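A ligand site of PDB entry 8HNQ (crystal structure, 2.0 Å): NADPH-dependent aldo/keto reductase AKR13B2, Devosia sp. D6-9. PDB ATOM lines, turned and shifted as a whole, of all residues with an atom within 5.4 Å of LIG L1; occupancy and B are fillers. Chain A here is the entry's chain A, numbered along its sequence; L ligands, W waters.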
ATOM      1  N   GLY A  31     -27.504  16.085 -25.111  1.00  0.00           N
ATOM      2  CA  GLY A  31     -26.129  15.621 -25.032  1.00  0.00           C
ATOM      3  C   GLY A  31     -26.071  14.132 -24.722  1.00  0.00           C
ATOM      4  O   GLY A  31     -26.623  13.683 -23.727  1.00  0.00           O
ATOM      5  N   ALA A  32     -25.422  13.356 -25.584  1.00  0.00           N
ATOM      6  CA  ALA A  32     -25.428  11.899 -25.495  1.00  0.00           C
ATOM      7  C   ALA A  32     -24.182  11.346 -24.812  1.00  0.00           C
ATOM      8  O   ALA A  32     -23.880  10.158 -24.959  1.00  0.00           O
ATOM      9  CB  ALA A  32     -25.602  11.297 -26.886  1.00  0.00           C
ATOM     10  N   MET A  33     -23.446  12.178 -24.079  1.00  0.00           N
ATOM     11  CA  MET A  33     -22.251  11.652 -23.396  1.00  0.00           C
ATOM     12  C   MET A  33     -22.611  10.761 -22.217  1.00  0.00           C
ATOM     13  O   MET A  33     -21.817   9.908 -21.821  1.00  0.00           O
ATOM     14  CB  MET A  33     -21.374  12.799 -22.905  1.00  0.00           C
ATOM     15  CG  MET A  33     -19.964  12.351 -22.533  1.00  0.00           C
ATOM     16  SD  MET A  33     -18.908  13.763 -22.077  1.00  0.00           S
ATOM     17  CE  MET A  33     -19.746  14.290 -20.588  1.00  0.00           C
ATOM     18  N   ARG A  34     -23.795  10.961 -21.623  1.00  0.00           N
ATOM     19  CA  ARG A  34     -24.124  10.318 -20.363  1.00  0.00           C
ATOM     20  C   ARG A  34     -24.800   8.955 -20.538  1.00  0.00           C
ATOM     21  O   ARG A  34     -25.114   8.318 -19.535  1.00  0.00           O
ATOM     22  CB  ARG A  34     -25.006  11.247 -19.528  1.00  0.00           C
ATOM     23  CG  ARG A  34     -24.382  12.630 -19.217  1.00  0.00           C
ATOM     24  CD  ARG A  34     -23.070  12.482 -18.415  1.00  0.00           C
ATOM     25  NE  ARG A  34     -22.337  13.751 -18.286  1.00  0.00           N
ATOM     26  CZ  ARG A  34     -21.312  13.937 -17.456  1.00  0.00           C
ATOM     27  NH1 ARG A  34     -20.887  12.944 -16.675  1.00  0.00           N
ATOM     28  NH2 ARG A  34     -20.700  15.125 -17.399  1.00  0.00           N
ATOM     29  N   ASP A  66     -25.962  15.373 -29.780  1.00  0.00           N
ATOM     30  CA  ASP A  66     -24.509  15.522 -29.830  1.00  0.00           C
ATOM     31  C   ASP A  66     -23.866  14.302 -29.206  1.00  0.00           C
ATOM     32  O   ASP A  66     -24.123  13.988 -28.043  1.00  0.00           O
ATOM     33  CB  ASP A  66     -24.049  16.777 -29.082  1.00  0.00           C
ATOM     34  CG  ASP A  66     -22.529  16.923 -29.109  1.00  0.00           C
ATOM     35  OD1 ASP A  66     -21.983  17.222 -30.190  1.00  0.00           O
ATOM     36  OD2 ASP A  66     -21.878  16.683 -28.068  1.00  0.00           O
ATOM     37  N   THR A  67     -23.002  13.631 -29.970  1.00  0.00           N
ATOM     38  CA  THR A  67     -22.258  12.485 -29.454  1.00  0.00           C
ATOM     39  C   THR A  67     -20.806  12.657 -29.878  1.00  0.00           C
ATOM     40  O   THR A  67     -20.350  13.741 -30.257  1.00  0.00           O
ATOM     41  CB  THR A  67     -22.906  11.178 -29.929  1.00  0.00           C
ATOM     42  OG1 THR A  67     -22.212  10.051 -29.376  1.00  0.00           O
ATOM     43  CG2 THR A  67     -22.908  11.059 -31.462  1.00  0.00           C
ATOM     44  N   TYR A  71     -17.132   8.810 -26.811  1.00  0.00           N
ATOM     45  CA  TYR A  71     -18.087   8.605 -25.718  1.00  0.00           C
ATOM     46  C   TYR A  71     -18.345   7.104 -25.575  1.00  0.00           C
ATOM     47  O   TYR A  71     -19.213   6.526 -26.238  1.00  0.00           O
ATOM     48  CB  TYR A  71     -19.387   9.372 -25.948  1.00  0.00           C
ATOM     49  CG  TYR A  71     -19.234  10.881 -25.946  1.00  0.00           C
ATOM     50  CD1 TYR A  71     -18.046  11.498 -25.518  1.00  0.00           C
ATOM     51  CD2 TYR A  71     -20.285  11.708 -26.386  1.00  0.00           C
ATOM     52  CE1 TYR A  71     -17.923  12.902 -25.523  1.00  0.00           C
ATOM     53  CE2 TYR A  71     -20.158  13.086 -26.405  1.00  0.00           C
ATOM     54  CZ  TYR A  71     -18.983  13.678 -25.977  1.00  0.00           C
ATOM     55  OH  TYR A  71     -18.882  15.062 -26.013  1.00  0.00           O
ATOM     56  N   LYS A  95     -17.996  13.698 -33.298  1.00  0.00           N
ATOM     57  CA  LYS A  95     -16.668  14.272 -33.129  1.00  0.00           C
ATOM     58  C   LYS A  95     -15.644  13.169 -33.321  1.00  0.00           C
ATOM     59  O   LYS A  95     -15.940  11.983 -33.133  1.00  0.00           O
ATOM     60  CB  LYS A  95     -16.456  14.887 -31.750  1.00  0.00           C
ATOM     61  CG  LYS A  95     -17.597  15.743 -31.183  1.00  0.00           C
ATOM     62  CD  LYS A  95     -17.231  16.221 -29.786  1.00  0.00           C
ATOM     63  CE  LYS A  95     -18.409  16.937 -29.124  1.00  0.00           C
ATOM     64  NZ  LYS A  95     -19.450  15.976 -28.643  1.00  0.00           N
ATOM     65  N   HIS A 137     -12.826  17.502 -32.074  1.00  0.00           N
ATOM     66  CA  HIS A 137     -13.107  17.450 -30.640  1.00  0.00           C
ATOM     67  C   HIS A 137     -12.169  18.375 -29.857  1.00  0.00           C
ATOM     68  O   HIS A 137     -12.612  19.107 -28.965  1.00  0.00           O
ATOM     69  CB  HIS A 137     -13.019  16.001 -30.145  1.00  0.00           C
ATOM     70  CG  HIS A 137     -13.809  15.727 -28.904  1.00  0.00           C
ATOM     71  ND1 HIS A 137     -14.269  14.461 -28.573  1.00  0.00           N
ATOM     72  CD2 HIS A 137     -14.223  16.548 -27.916  1.00  0.00           C
ATOM     73  CE1 HIS A 137     -14.929  14.517 -27.435  1.00  0.00           C
ATOM     74  NE2 HIS A 137     -14.909  15.770 -27.007  1.00  0.00           N
ATOM     75  N   ARG A 138     -10.892  18.399 -30.227  1.00  0.00           N
ATOM     76  CA  ARG A 138      -9.930  19.390 -29.764  1.00  0.00           C
ATOM     77  C   ARG A 138      -8.903  19.597 -30.862  1.00  0.00           C
ATOM     78  O   ARG A 138      -8.546  18.656 -31.566  1.00  0.00           O
ATOM     79  CB  ARG A 138      -9.181  18.965 -28.487  1.00  0.00           C
ATOM     80  CG  ARG A 138      -9.993  18.990 -27.208  1.00  0.00           C
ATOM     81  CD  ARG A 138     -10.368  20.409 -26.832  1.00  0.00           C
ATOM     82  NE  ARG A 138     -10.941  20.469 -25.490  1.00  0.00           N
ATOM     83  CZ  ARG A 138     -12.219  20.206 -25.209  1.00  0.00           C
ATOM     84  NH1 ARG A 138     -13.061  19.859 -26.179  1.00  0.00           N
ATOM     85  NH2 ARG A 138     -12.654  20.281 -23.962  1.00  0.00           N
ATOM     86  N   SER A 167     -14.406  22.860 -31.199  1.00  0.00           N
ATOM     87  CA  SER A 167     -14.749  22.688 -29.793  1.00  0.00           C
ATOM     88  C   SER A 167     -13.646  23.225 -28.890  1.00  0.00           C
ATOM     89  O   SER A 167     -12.463  22.915 -29.078  1.00  0.00           O
ATOM     90  CB  SER A 167     -15.043  21.207 -29.487  1.00  0.00           C
ATOM     91  OG  SER A 167     -15.402  21.051 -28.116  1.00  0.00           O
ATOM     92  N   GLN A 187     -18.357  24.448 -29.973  1.00  0.00           N
ATOM     93  CA  GLN A 187     -18.866  23.827 -28.759  1.00  0.00           C
ATOM     94  C   GLN A 187     -17.867  24.116 -27.644  1.00  0.00           C
ATOM     95  O   GLN A 187     -16.823  23.450 -27.539  1.00  0.00           O
ATOM     96  CB  GLN A 187     -19.087  22.321 -28.951  1.00  0.00           C
ATOM     97  CG  GLN A 187     -19.699  21.674 -27.718  1.00  0.00           C
ATOM     98  CD  GLN A 187     -20.104  20.226 -27.936  1.00  0.00           C
ATOM     99  OE1 GLN A 187     -19.980  19.415 -27.044  1.00  0.00           O
ATOM    100  NE2 GLN A 187     -20.609  19.924 -29.127  1.00  0.00           N
ATOM    101  N   PRO A 213     -23.207  25.173 -25.954  1.00  0.00           N
ATOM    102  CA  PRO A 213     -22.545  25.184 -24.635  1.00  0.00           C
ATOM    103  C   PRO A 213     -22.475  23.770 -24.082  1.00  0.00           C
ATOM    104  O   PRO A 213     -23.499  23.110 -23.911  1.00  0.00           O
ATOM    105  CB  PRO A 213     -23.454  26.072 -23.794  1.00  0.00           C
ATOM    106  CG  PRO A 213     -24.808  25.820 -24.364  1.00  0.00           C
ATOM    107  CD  PRO A 213     -24.616  25.568 -25.855  1.00  0.00           C
ATOM    108  N   TRP A 214     -21.265  23.306 -23.797  1.00  0.00           N
ATOM    109  CA  TRP A 214     -21.223  22.042 -23.088  1.00  0.00           C
ATOM    110  C   TRP A 214     -21.152  22.300 -21.581  1.00  0.00           C
ATOM    111  O   TRP A 214     -20.840  23.401 -21.133  1.00  0.00           O
ATOM    112  CB  TRP A 214     -20.088  21.126 -23.567  1.00  0.00           C
ATOM    113  CG  TRP A 214     -18.625  21.550 -23.507  1.00  0.00           C
ATOM    114  CD1 TRP A 214     -17.873  22.084 -24.522  1.00  0.00           C
ATOM    115  CD2 TRP A 214     -17.711  21.332 -22.416  1.00  0.00           C
ATOM    116  NE1 TRP A 214     -16.566  22.256 -24.112  1.00  0.00           N
ATOM    117  CE2 TRP A 214     -16.435  21.804 -22.824  1.00  0.00           C
ATOM    118  CE3 TRP A 214     -17.860  20.818 -21.113  1.00  0.00           C
ATOM    119  CZ2 TRP A 214     -15.313  21.771 -21.991  1.00  0.00           C
ATOM    120  CZ3 TRP A 214     -16.729  20.766 -20.282  1.00  0.00           C
ATOM    121  CH2 TRP A 214     -15.477  21.257 -20.732  1.00  0.00           C
ATOM    122  N   ALA A 215     -21.497  21.264 -20.821  1.00  0.00           N
ATOM    123  CA  ALA A 215     -21.842  21.396 -19.405  1.00  0.00           C
ATOM    124  C   ALA A 215     -22.824  22.558 -19.182  1.00  0.00           C
ATOM    125  O   ALA A 215     -22.549  23.456 -18.379  1.00  0.00           O
ATOM    126  CB  ALA A 215     -20.592  21.576 -18.546  1.00  0.00           C
ATOM    127  N   PRO A 216     -23.968  22.555 -19.875  1.00  0.00           N
ATOM    128  CA  PRO A 216     -24.924  23.670 -19.707  1.00  0.00           C
ATOM    129  C   PRO A 216     -25.603  23.650 -18.353  1.00  0.00           C
ATOM    130  O   PRO A 216     -26.131  24.687 -17.931  1.00  0.00           O
ATOM    131  CB  PRO A 216     -25.940  23.438 -20.825  1.00  0.00           C
ATOM    132  CG  PRO A 216     -25.976  21.956 -20.969  1.00  0.00           C
ATOM    133  CD  PRO A 216     -24.551  21.459 -20.672  1.00  0.00           C
ATOM    134  N   LEU A 217     -25.658  22.493 -17.695  1.00  0.00           N
ATOM    135  CA  LEU A 217     -26.126  22.378 -16.323  1.00  0.00           C
ATOM    136  C   LEU A 217     -24.972  22.338 -15.342  1.00  0.00           C
ATOM    137  O   LEU A 217     -25.137  21.816 -14.236  1.00  0.00           O
ATOM    138  CB  LEU A 217     -27.004  21.131 -16.157  1.00  0.00           C
ATOM    139  CG  LEU A 217     -28.299  21.006 -16.982  1.00  0.00           C
ATOM    140  CD1 LEU A 217     -28.892  19.609 -16.803  1.00  0.00           C
ATOM    141  CD2 LEU A 217     -29.316  22.068 -16.567  1.00  0.00           C
ATOM    142  N   ALA A 218     -23.803  22.865 -15.734  1.00  0.00           N
ATOM    143  CA  ALA A 218     -22.539  22.798 -14.965  1.00  0.00           C
ATOM    144  C   ALA A 218     -22.303  21.401 -14.379  1.00  0.00           C
ATOM    145  O   ALA A 218     -22.005  21.235 -13.190  1.00  0.00           O
ATOM    146  CB  ALA A 218     -22.479  23.882 -13.889  1.00  0.00           C
ATOM    147  N   SER A 219     -22.454  20.382 -15.243  1.00  0.00           N
ATOM    148  CA  SER A 219     -22.296  18.976 -14.870  1.00  0.00           C
ATOM    149  C   SER A 219     -23.270  18.558 -13.770  1.00  0.00           C
ATOM    150  O   SER A 219     -22.943  17.721 -12.923  1.00  0.00           O
ATOM    151  CB  SER A 219     -20.855  18.655 -14.428  1.00  0.00           C
ATOM    152  OG  SER A 219     -19.917  19.220 -15.324  1.00  0.00           O
ATOM    153  N   GLY A 220     -24.477  19.134 -13.777  1.00  0.00           N
ATOM    154  CA  GLY A 220     -25.500  18.836 -12.805  1.00  0.00           C
ATOM    155  C   GLY A 220     -25.398  19.588 -11.494  1.00  0.00           C
ATOM    156  O   GLY A 220     -26.278  19.423 -10.639  1.00  0.00           O
ATOM    157  N   ILE A 257     -27.154  21.498 -24.987  1.00  0.00           N
ATOM    158  CA  ILE A 257     -27.228  20.043 -25.128  1.00  0.00           C
ATOM    159  C   ILE A 257     -27.116  19.393 -23.759  1.00  0.00           C
ATOM    160  O   ILE A 257     -26.176  18.615 -23.521  1.00  0.00           O
ATOM    161  CB  ILE A 257     -26.142  19.533 -26.103  1.00  0.00           C
ATOM    162  CG1 ILE A 257     -24.779  20.138 -25.773  1.00  0.00           C
ATOM    163  CG2 ILE A 257     -26.537  19.860 -27.567  1.00  0.00           C
ATOM    164  CD1 ILE A 257     -23.593  19.394 -26.425  1.00  0.00           C
ATOM    165  N   PRO A 258     -28.055  19.635 -22.843  1.00  0.00           N
ATOM    166  CA  PRO A 258     -27.985  18.982 -21.522  1.00  0.00           C
ATOM    167  C   PRO A 258     -27.932  17.461 -21.675  1.00  0.00           C
ATOM    168  O   PRO A 258     -28.618  16.882 -22.518  1.00  0.00           O
ATOM    169  CB  PRO A 258     -29.280  19.440 -20.820  1.00  0.00           C
ATOM    170  CG  PRO A 258     -30.217  19.757 -21.973  1.00  0.00           C
ATOM    171  CD  PRO A 258     -29.308  20.385 -23.010  1.00  0.00           C
ATOM    172  N   GLY A 259     -27.098  16.837 -20.870  1.00  0.00           N
ATOM    173  CA  GLY A 259     -26.844  15.402 -20.960  1.00  0.00           C
ATOM    174  C   GLY A 259     -27.495  14.680 -19.809  1.00  0.00           C
ATOM    175  O   GLY A 259     -27.436  15.126 -18.664  1.00  0.00           O
ATOM    176  N   THR A 260     -28.140  13.555 -20.114  1.00  0.00           N
ATOM    177  CA  THR A 260     -28.725  12.741 -19.071  1.00  0.00           C
ATOM    178  C   THR A 260     -28.845  11.309 -19.576  1.00  0.00           C
ATOM    179  O   THR A 260     -28.876  11.056 -20.770  1.00  0.00           O
ATOM    180  CB  THR A 260     -30.091  13.268 -18.636  1.00  0.00           C
ATOM    181  OG1 THR A 260     -30.589  12.416 -17.586  1.00  0.00           O
ATOM    182  CG2 THR A 260     -31.073  13.257 -19.811  1.00  0.00           C
ATOM    183  N   GLY A 261     -28.905  10.380 -18.623  1.00  0.00           N
ATOM    184  CA  GLY A 261     -29.245   9.000 -18.907  1.00  0.00           C
ATOM    185  C   GLY A 261     -30.584   8.579 -18.315  1.00  0.00           C
ATOM    186  O   GLY A 261     -30.846   7.376 -18.231  1.00  0.00           O
ATOM    187  N   LYS A 262     -31.433   9.528 -17.923  1.00  0.00           N
ATOM    188  CA  LYS A 262     -32.730   9.205 -17.309  1.00  0.00           C
ATOM    189  C   LYS A 262     -33.866   9.939 -18.020  1.00  0.00           C
ATOM    190  O   LYS A 262     -33.772  11.142 -18.293  1.00  0.00           O
ATOM    191  CB  LYS A 262     -32.741   9.562 -15.814  1.00  0.00           C
ATOM    192  CG  LYS A 262     -31.746   8.758 -14.975  1.00  0.00           C
ATOM    193  CD  LYS A 262     -31.519   9.452 -13.630  1.00  0.00           C
ATOM    194  CE  LYS A 262     -30.602   8.626 -12.707  1.00  0.00           C
ATOM    195  NZ  LYS A 262     -29.167   8.606 -13.145  1.00  0.00           N
ATOM    196  N   ALA A 264     -36.834  10.781 -16.894  1.00  0.00           N
ATOM    197  CA  ALA A 264     -37.429  11.839 -16.091  1.00  0.00           C
ATOM    198  C   ALA A 264     -36.622  13.132 -16.192  1.00  0.00           C
ATOM    199  O   ALA A 264     -37.195  14.238 -16.238  1.00  0.00           O
ATOM    200  CB  ALA A 264     -37.554  11.410 -14.621  1.00  0.00           C
ATOM    201  N   HIS A 265     -35.287  13.032 -16.239  1.00  0.00           N
ATOM    202  CA  HIS A 265     -34.454  14.223 -16.338  1.00  0.00           C
ATOM    203  C   HIS A 265     -34.492  14.811 -17.740  1.00  0.00           C
ATOM    204  O   HIS A 265     -34.483  16.034 -17.906  1.00  0.00           O
ATOM    205  CB  HIS A 265     -33.021  13.882 -15.925  1.00  0.00           C
ATOM    206  CG  HIS A 265     -32.886  13.516 -14.480  1.00  0.00           C
ATOM    207  ND1 HIS A 265     -31.696  13.151 -13.902  1.00  0.00           N
ATOM    208  CD2 HIS A 265     -33.815  13.457 -13.497  1.00  0.00           C
ATOM    209  CE1 HIS A 265     -31.888  12.876 -12.625  1.00  0.00           C
ATOM    210  NE2 HIS A 265     -33.169  13.060 -12.341  1.00  0.00           N
ATOM    211  N   LEU A 266     -34.516  13.956 -18.762  1.00  0.00           N
ATOM    212  CA  LEU A 266     -34.699  14.419 -20.124  1.00  0.00           C
ATOM    213  C   LEU A 266     -35.971  15.268 -20.246  1.00  0.00           C
ATOM    214  O   LEU A 266     -35.949  16.363 -20.822  1.00  0.00           O
ATOM    215  CB  LEU A 266     -34.738  13.229 -21.086  1.00  0.00           C
ATOM    216  CG  LEU A 266     -35.148  13.596 -22.521  1.00  0.00           C
ATOM    217  CD1 LEU A 266     -34.000  14.324 -23.219  1.00  0.00           C
ATOM    218  CD2 LEU A 266     -35.572  12.361 -23.318  1.00  0.00           C
ATOM    219  N   GLU A 268     -37.585  16.876 -17.876  1.00  0.00           N
ATOM    220  CA  GLU A 268     -37.384  18.123 -17.162  1.00  0.00           C
ATOM    221  C   GLU A 268     -36.511  19.099 -17.963  1.00  0.00           C
ATOM    222  O   GLU A 268     -36.769  20.311 -17.993  1.00  0.00           O
ATOM    223  CB  GLU A 268     -36.751  17.839 -15.795  1.00  0.00           C
ATOM    224  CG  GLU A 268     -36.160  19.066 -15.169  1.00  0.00           C
ATOM    225  CD  GLU A 268     -35.507  18.779 -13.834  1.00  0.00           C
ATOM    226  OE1 GLU A 268     -34.721  19.647 -13.361  1.00  0.00           O
ATOM    227  OE2 GLU A 268     -35.789  17.692 -13.258  1.00  0.00           O
ATOM    228  N   ASN A 269     -35.484  18.574 -18.635  1.00  0.00           N
ATOM    229  CA  ASN A 269     -34.589  19.450 -19.375  1.00  0.00           C
ATOM    230  C   ASN A 269     -35.295  20.061 -20.580  1.00  0.00           C
ATOM    231  O   ASN A 269     -35.150  21.261 -20.856  1.00  0.00           O
ATOM    232  CB  ASN A 269     -33.353  18.673 -19.809  1.00  0.00           C
ATOM    233  CG  ASN A 269     -32.487  18.290 -18.639  1.00  0.00           C
ATOM    234  OD1 ASN A 269     -32.677  18.786 -17.525  1.00  0.00           O
ATOM    235  ND2 ASN A 269     -31.554  17.361 -18.858  1.00  0.00           N
HETATM  236  P1  LIG L   1     -24.405  18.739 -18.015  1.00  0.00           P
HETATM  237  O1  LIG L   1     -24.239  20.194 -17.663  1.00  0.00           O
HETATM  238  O2  LIG L   1     -25.385  18.503 -19.179  1.00  0.00           O
HETATM  239  O3  LIG L   1     -24.950  17.921 -16.664  1.00  0.00           O
HETATM  240  C1  LIG L   1     -25.008  16.530 -16.832  1.00  0.00           C
HETATM  241  C2  LIG L   1     -25.179  15.973 -15.393  1.00  0.00           C
HETATM  242  O4  LIG L   1     -26.294  16.487 -14.912  1.00  0.00           O
HETATM  243  C3  LIG L   1     -25.354  14.484 -15.478  1.00  0.00           C
HETATM  244  O5  LIG L   1     -24.658  13.917 -14.438  1.00  0.00           O
HETATM  245  C4  LIG L   1     -26.878  14.269 -15.287  1.00  0.00           C
HETATM  246  O6  LIG L   1     -27.051  12.999 -14.497  1.00  0.00           O
HETATM  247  C5  LIG L   1     -27.301  15.276 -14.595  1.00  0.00           C
HETATM  248  N1  LIG L   1     -28.633  15.772 -15.052  1.00  0.00           N
HETATM  249  C6  LIG L   1     -29.049  16.127 -16.281  1.00  0.00           C
HETATM  250  N2  LIG L   1     -30.331  16.527 -16.178  1.00  0.00           N
HETATM  251  C7  LIG L   1     -30.688  16.433 -14.877  1.00  0.00           C
HETATM  252  C8  LIG L   1     -31.876  16.724 -14.239  1.00  0.00           C
HETATM  253  N3  LIG L   1     -33.034  17.191 -14.828  1.00  0.00           N
HETATM  254  N4  LIG L   1     -31.981  16.554 -12.921  1.00  0.00           N
HETATM  255  C9  LIG L   1     -30.911  16.078 -12.195  1.00  0.00           C
HETATM  256  N5  LIG L   1     -29.746  15.791 -12.825  1.00  0.00           N
HETATM  257  C10 LIG L   1     -29.638  15.975 -14.167  1.00  0.00           C
HETATM  258  O7  LIG L   1     -22.957  18.114 -18.314  1.00  0.00           O
HETATM  259  P2  LIG L   1     -22.478  17.290 -19.673  1.00  0.00           P
HETATM  260  O8  LIG L   1     -23.286  16.060 -19.873  1.00  0.00           O
HETATM  261  O9  LIG L   1     -21.022  16.959 -19.440  1.00  0.00           O
HETATM  262  O10 LIG L   1     -22.616  18.321 -20.966  1.00  0.00           O
HETATM  263  C11 LIG L   1     -23.720  18.136 -21.840  1.00  0.00           C
HETATM  264  C12 LIG L   1     -23.189  17.588 -23.164  1.00  0.00           C
HETATM  265  O11 LIG L   1     -22.206  18.363 -23.637  1.00  0.00           O
HETATM  266  C13 LIG L   1     -22.546  16.199 -22.983  1.00  0.00           C
HETATM  267  O12 LIG L   1     -23.451  15.188 -22.939  1.00  0.00           O
HETATM  268  C14 LIG L   1     -21.621  16.146 -24.245  1.00  0.00           C
HETATM  269  O13 LIG L   1     -22.516  15.835 -25.417  1.00  0.00           O
HETATM  270  C15 LIG L   1     -21.168  17.385 -24.404  1.00  0.00           C
HETATM  271  N6  LIG L   1     -19.834  17.639 -23.844  1.00  0.00           N
HETATM  272  C16 LIG L   1     -18.859  18.074 -24.662  1.00  0.00           C
HETATM  273  C17 LIG L   1     -17.591  18.339 -24.179  1.00  0.00           C
HETATM  274  C18 LIG L   1     -16.514  18.855 -25.199  1.00  0.00           C
HETATM  275  O14 LIG L   1     -15.389  19.026 -24.856  1.00  0.00           O
HETATM  276  N7  LIG L   1     -16.913  19.137 -26.500  1.00  0.00           N
HETATM  277  C19 LIG L   1     -17.315  18.153 -22.857  1.00  0.00           C
HETATM  278  C20 LIG L   1     -18.315  17.724 -22.015  1.00  0.00           C
HETATM  279  C21 LIG L   1     -19.568  17.467 -22.507  1.00  0.00           C
HETATM  280  P3  LIG L   1     -28.243  11.952 -14.901  1.00  0.00           P
HETATM  281  O15 LIG L   1     -29.478  12.757 -15.265  1.00  0.00           O
HETATM  282  O16 LIG L   1     -27.819  11.061 -16.093  1.00  0.00           O
HETATM  283  O17 LIG L   1     -28.468  11.079 -13.677  1.00  0.00           O
HETATM  284  C1  LG2 L   2     -16.210  15.892 -19.526  1.00  0.00           C
HETATM  285  O1  LG2 L   2     -15.261  16.533 -18.725  1.00  0.00           O
HETATM  286  C2  LG2 L   2     -15.833  17.515 -17.905  1.00  0.00           C
HETATM  287  C3  LG2 L   2     -14.735  18.285 -17.172  1.00  0.00           C
HETATM  288  O2  LG2 L   2     -13.862  18.837 -18.102  1.00  0.00           O
HETATM  289  C4  LG2 L   2     -12.830  19.474 -17.398  1.00  0.00           C
HETATM  290  C5  LG2 L   2     -11.926  20.232 -18.360  1.00  0.00           C
HETATM  291  O3  LG2 L   2     -11.397  19.336 -19.285  1.00  0.00           O
HETATM  292  C6  LG2 L   2     -10.315  19.915 -19.939  1.00  0.00           C
HETATM  293  C7  LG2 L   2      -9.728  18.892 -20.912  1.00  0.00           C
HETATM  294  O4  LG2 L   2     -10.737  18.386 -21.743  1.00  0.00           O
HETATM  295  C8  LG2 L   2     -10.169  17.478 -22.636  1.00  0.00           C
HETATM  296  C9  LG2 L   2     -11.304  16.854 -23.455  1.00  0.00           C
HETATM  297  O5  LG2 L   2     -12.306  16.402 -22.593  1.00  0.00           O
HETATM  298  C10 LG2 L   2     -13.420  16.000 -23.347  1.00  0.00           C
HETATM  299  C11 LG2 L   2     -14.283  15.075 -22.490  1.00  0.00           C
HETATM  300  O6  LG2 L   2     -14.760  15.809 -21.404  1.00  0.00           O
HETATM  301  C12 LG2 L   2     -15.513  14.995 -20.551  1.00  0.00           C
HETATM  302  O   HOH W   1     -26.079  10.465 -12.477  1.00  0.00           O
HETATM  303  O   HOH W   2     -27.967  14.191 -11.090  1.00  0.00           O
HETATM  304  O   HOH W   3     -16.492  15.677 -24.723  1.00  0.00           O
HETATM  305  O   HOH W   4     -32.642  20.526 -15.581  1.00  0.00           O
HETATM  306  O   HOH W   5     -28.467  18.290 -11.441  1.00  0.00           O
HETATM  307  O   HOH W   6     -27.733   8.304 -15.817  1.00  0.00           O
HETATM  308  O   HOH W   7     -34.225  16.430 -11.088  1.00  0.00           O
HETATM  309  O   HOH W   8     -21.930  14.662 -13.896  1.00  0.00           O
HETATM  310  O   HOH W   9     -19.120  18.127 -17.861  1.00  0.00           O
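An oxygen (O15) of LIG L1 sits at hydrogen-bond distance from the side-chain hydroxyl (OG1) of Thr 260, at 2.6 Å. The side-chain amino group of Lys 262 is in salt-bridge range of an oxygen (O17) of LIG L1, 2.6 Å away. ND1 of His 265 lies within hydrogen-bond range of O15 of LIG L1, at 2.6 Å. An oxygen (O1) of LIG L1 lies within hydrogen-bond range of the backbone NH (N) of Leu 217 (2.7 Å). An oxygen (O9) of LIG L1 is in salt-bridge range of the guanidinium group (NH2) of Arg 34, 2.8 Å away. An oxygen (O14) of LIG L1 is in hydrogen-bond range of the guanidinium group (NH1) of Arg 138 (2.8 Å). The backbone NH of Gly 261 is in hydrogen-bond range of an oxygen (O16) of LIG L1, at 2.8 Å. OD2 of Asp 66 lies within hydrogen-bond range of O13 of LIG L1. The side-chain hydroxyl of Ser 167 lies within hydrogen-bond range of a nitrogen (N7) of LIG L1, at 2.9 Å. O2 of LIG L1 sits at hydrogen-bond distance from N of Gly 259, 2.9 Å away. The side-chain amide oxygen of Gln 187 lies close to a nitrogen (N7) of LIG L1 (3.1 Å). An oxygen (O1) of LIG L1 sits at hydrogen-bond distance from the backbone NH (N) of Ser 219. The side-chain amide nitrogen (ND2) of Asn 269 sits at hydrogen-bond distance from a nitrogen (N2) of LIG L1 (3.1 Å). OE2 of Glu 268 lies close to N3 of LIG L1, 3.2 Å away. An oxygen (O10) of LIG L1 sits at hydrogen-bond distance from the backbone NH of Ala 215, 3.2 Å away. O12 of LIG L1 sits close to N of Met 33 (3.2 Å). The backbone NH of Gly 220 lies within hydrogen-bond range of an oxygen (O3) of LIG L1. The backbone NH of Ala 218 sits at hydrogen-bond distance from an oxygen (O1) of LIG L1. An oxygen (O4) of LG2 L2 lies within hydrogen-bond range of the guanidinium group (NH2) of Arg 138.
The backbone nitrogen (N) of Pro 216 sits close to an oxygen (O1) of LIG L1, 3.2 Å away. Gly 31 touches LIG L1. Ala 32 touches LIG L1 (N to O12, 3.8 Å). OH of Tyr 71 touches C16 of LIG L1, at 3.3 Å. Lys 95 touches LIG L1 (CE to N7, 3.7 Å). His 137 touches LIG L1 (NE2 to C18, 3.9 Å). CE3 of Trp 214 touches C19 of LIG L1, at 3.2 Å. O of Ile 257 touches C11 of LIG L1, 3.0 Å away. Pro 258 touches LIG L1. Hydrophobic or aromatic side chains that line LIG L1: Met 33, Tyr 71, His 137, Trp 214, Ala 215, Pro 216, Leu 217, Ile 257 and His 265. Of the 31 residues printed, 27 come within 4 Å of LIG L1. The nearest printed residue that does not touch LIG L1 is Pro 213 (4.9 Å).
Water W9 lies within hydrogen-bond range of an oxygen (O9) of LIG L1 (2.7 Å), the side-chain hydroxyl of Ser 219 (2.9 Å) and the guanidinium group of Arg 34 (3.4 Å). Water W6 bridges O16 of LIG L1 (2.8 Å) and NZ of Lys 262 (3.0 Å). Water W8 lies within hydrogen-bond range of O5 of LIG L1 (2.9 Å), O of Ser 219 (3.4 Å) and NH1 of Arg 34 (3.4 Å). Water W7 lies within hydrogen-bond range of a nitrogen (N4) of LIG L1 (2.9 Å) and the side-chain carboxylate of Glu 268 (3.0 Å). Water W3 bridges NE2 of His 137 (2.8 Å) and OH of Tyr 71 (2.8 Å). Water W5 lies within hydrogen-bond range of the backbone carbonyl oxygen of Gly 220 and a nitrogen (N5) of LIG L1.
O of His 265 lies close to OD1 of Asn 269, at 3.3 Å. NH1 of Arg 138 is in hydrogen-bond range of OG of Ser 167, at 3.3 Å. NE2 of Gln 187 sits at hydrogen-bond distance from OD1 of Asp 66, 3.2 Å away. The side-chain carboxylate (OD2) of Asp 66 is in salt-bridge range of the side-chain amino group (NZ) of Lys 95. The backbone carbonyl oxygen (O) of Asp 66 lies within hydrogen-bond range of the backbone NH (N) of Ala 32 (2.9 Å). OH of Tyr 71 lies within hydrogen-bond range of NZ of Lys 95 (2.8 Å). The backbone NH of Gly 31 lies within hydrogen-bond range of the backbone carbonyl oxygen of Pro 258 (2.9 Å). The side-chain amino group (NZ) of Lys 95 lies within hydrogen-bond range of the backbone carbonyl oxygen (O) of Thr 67 (2.9 Å).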
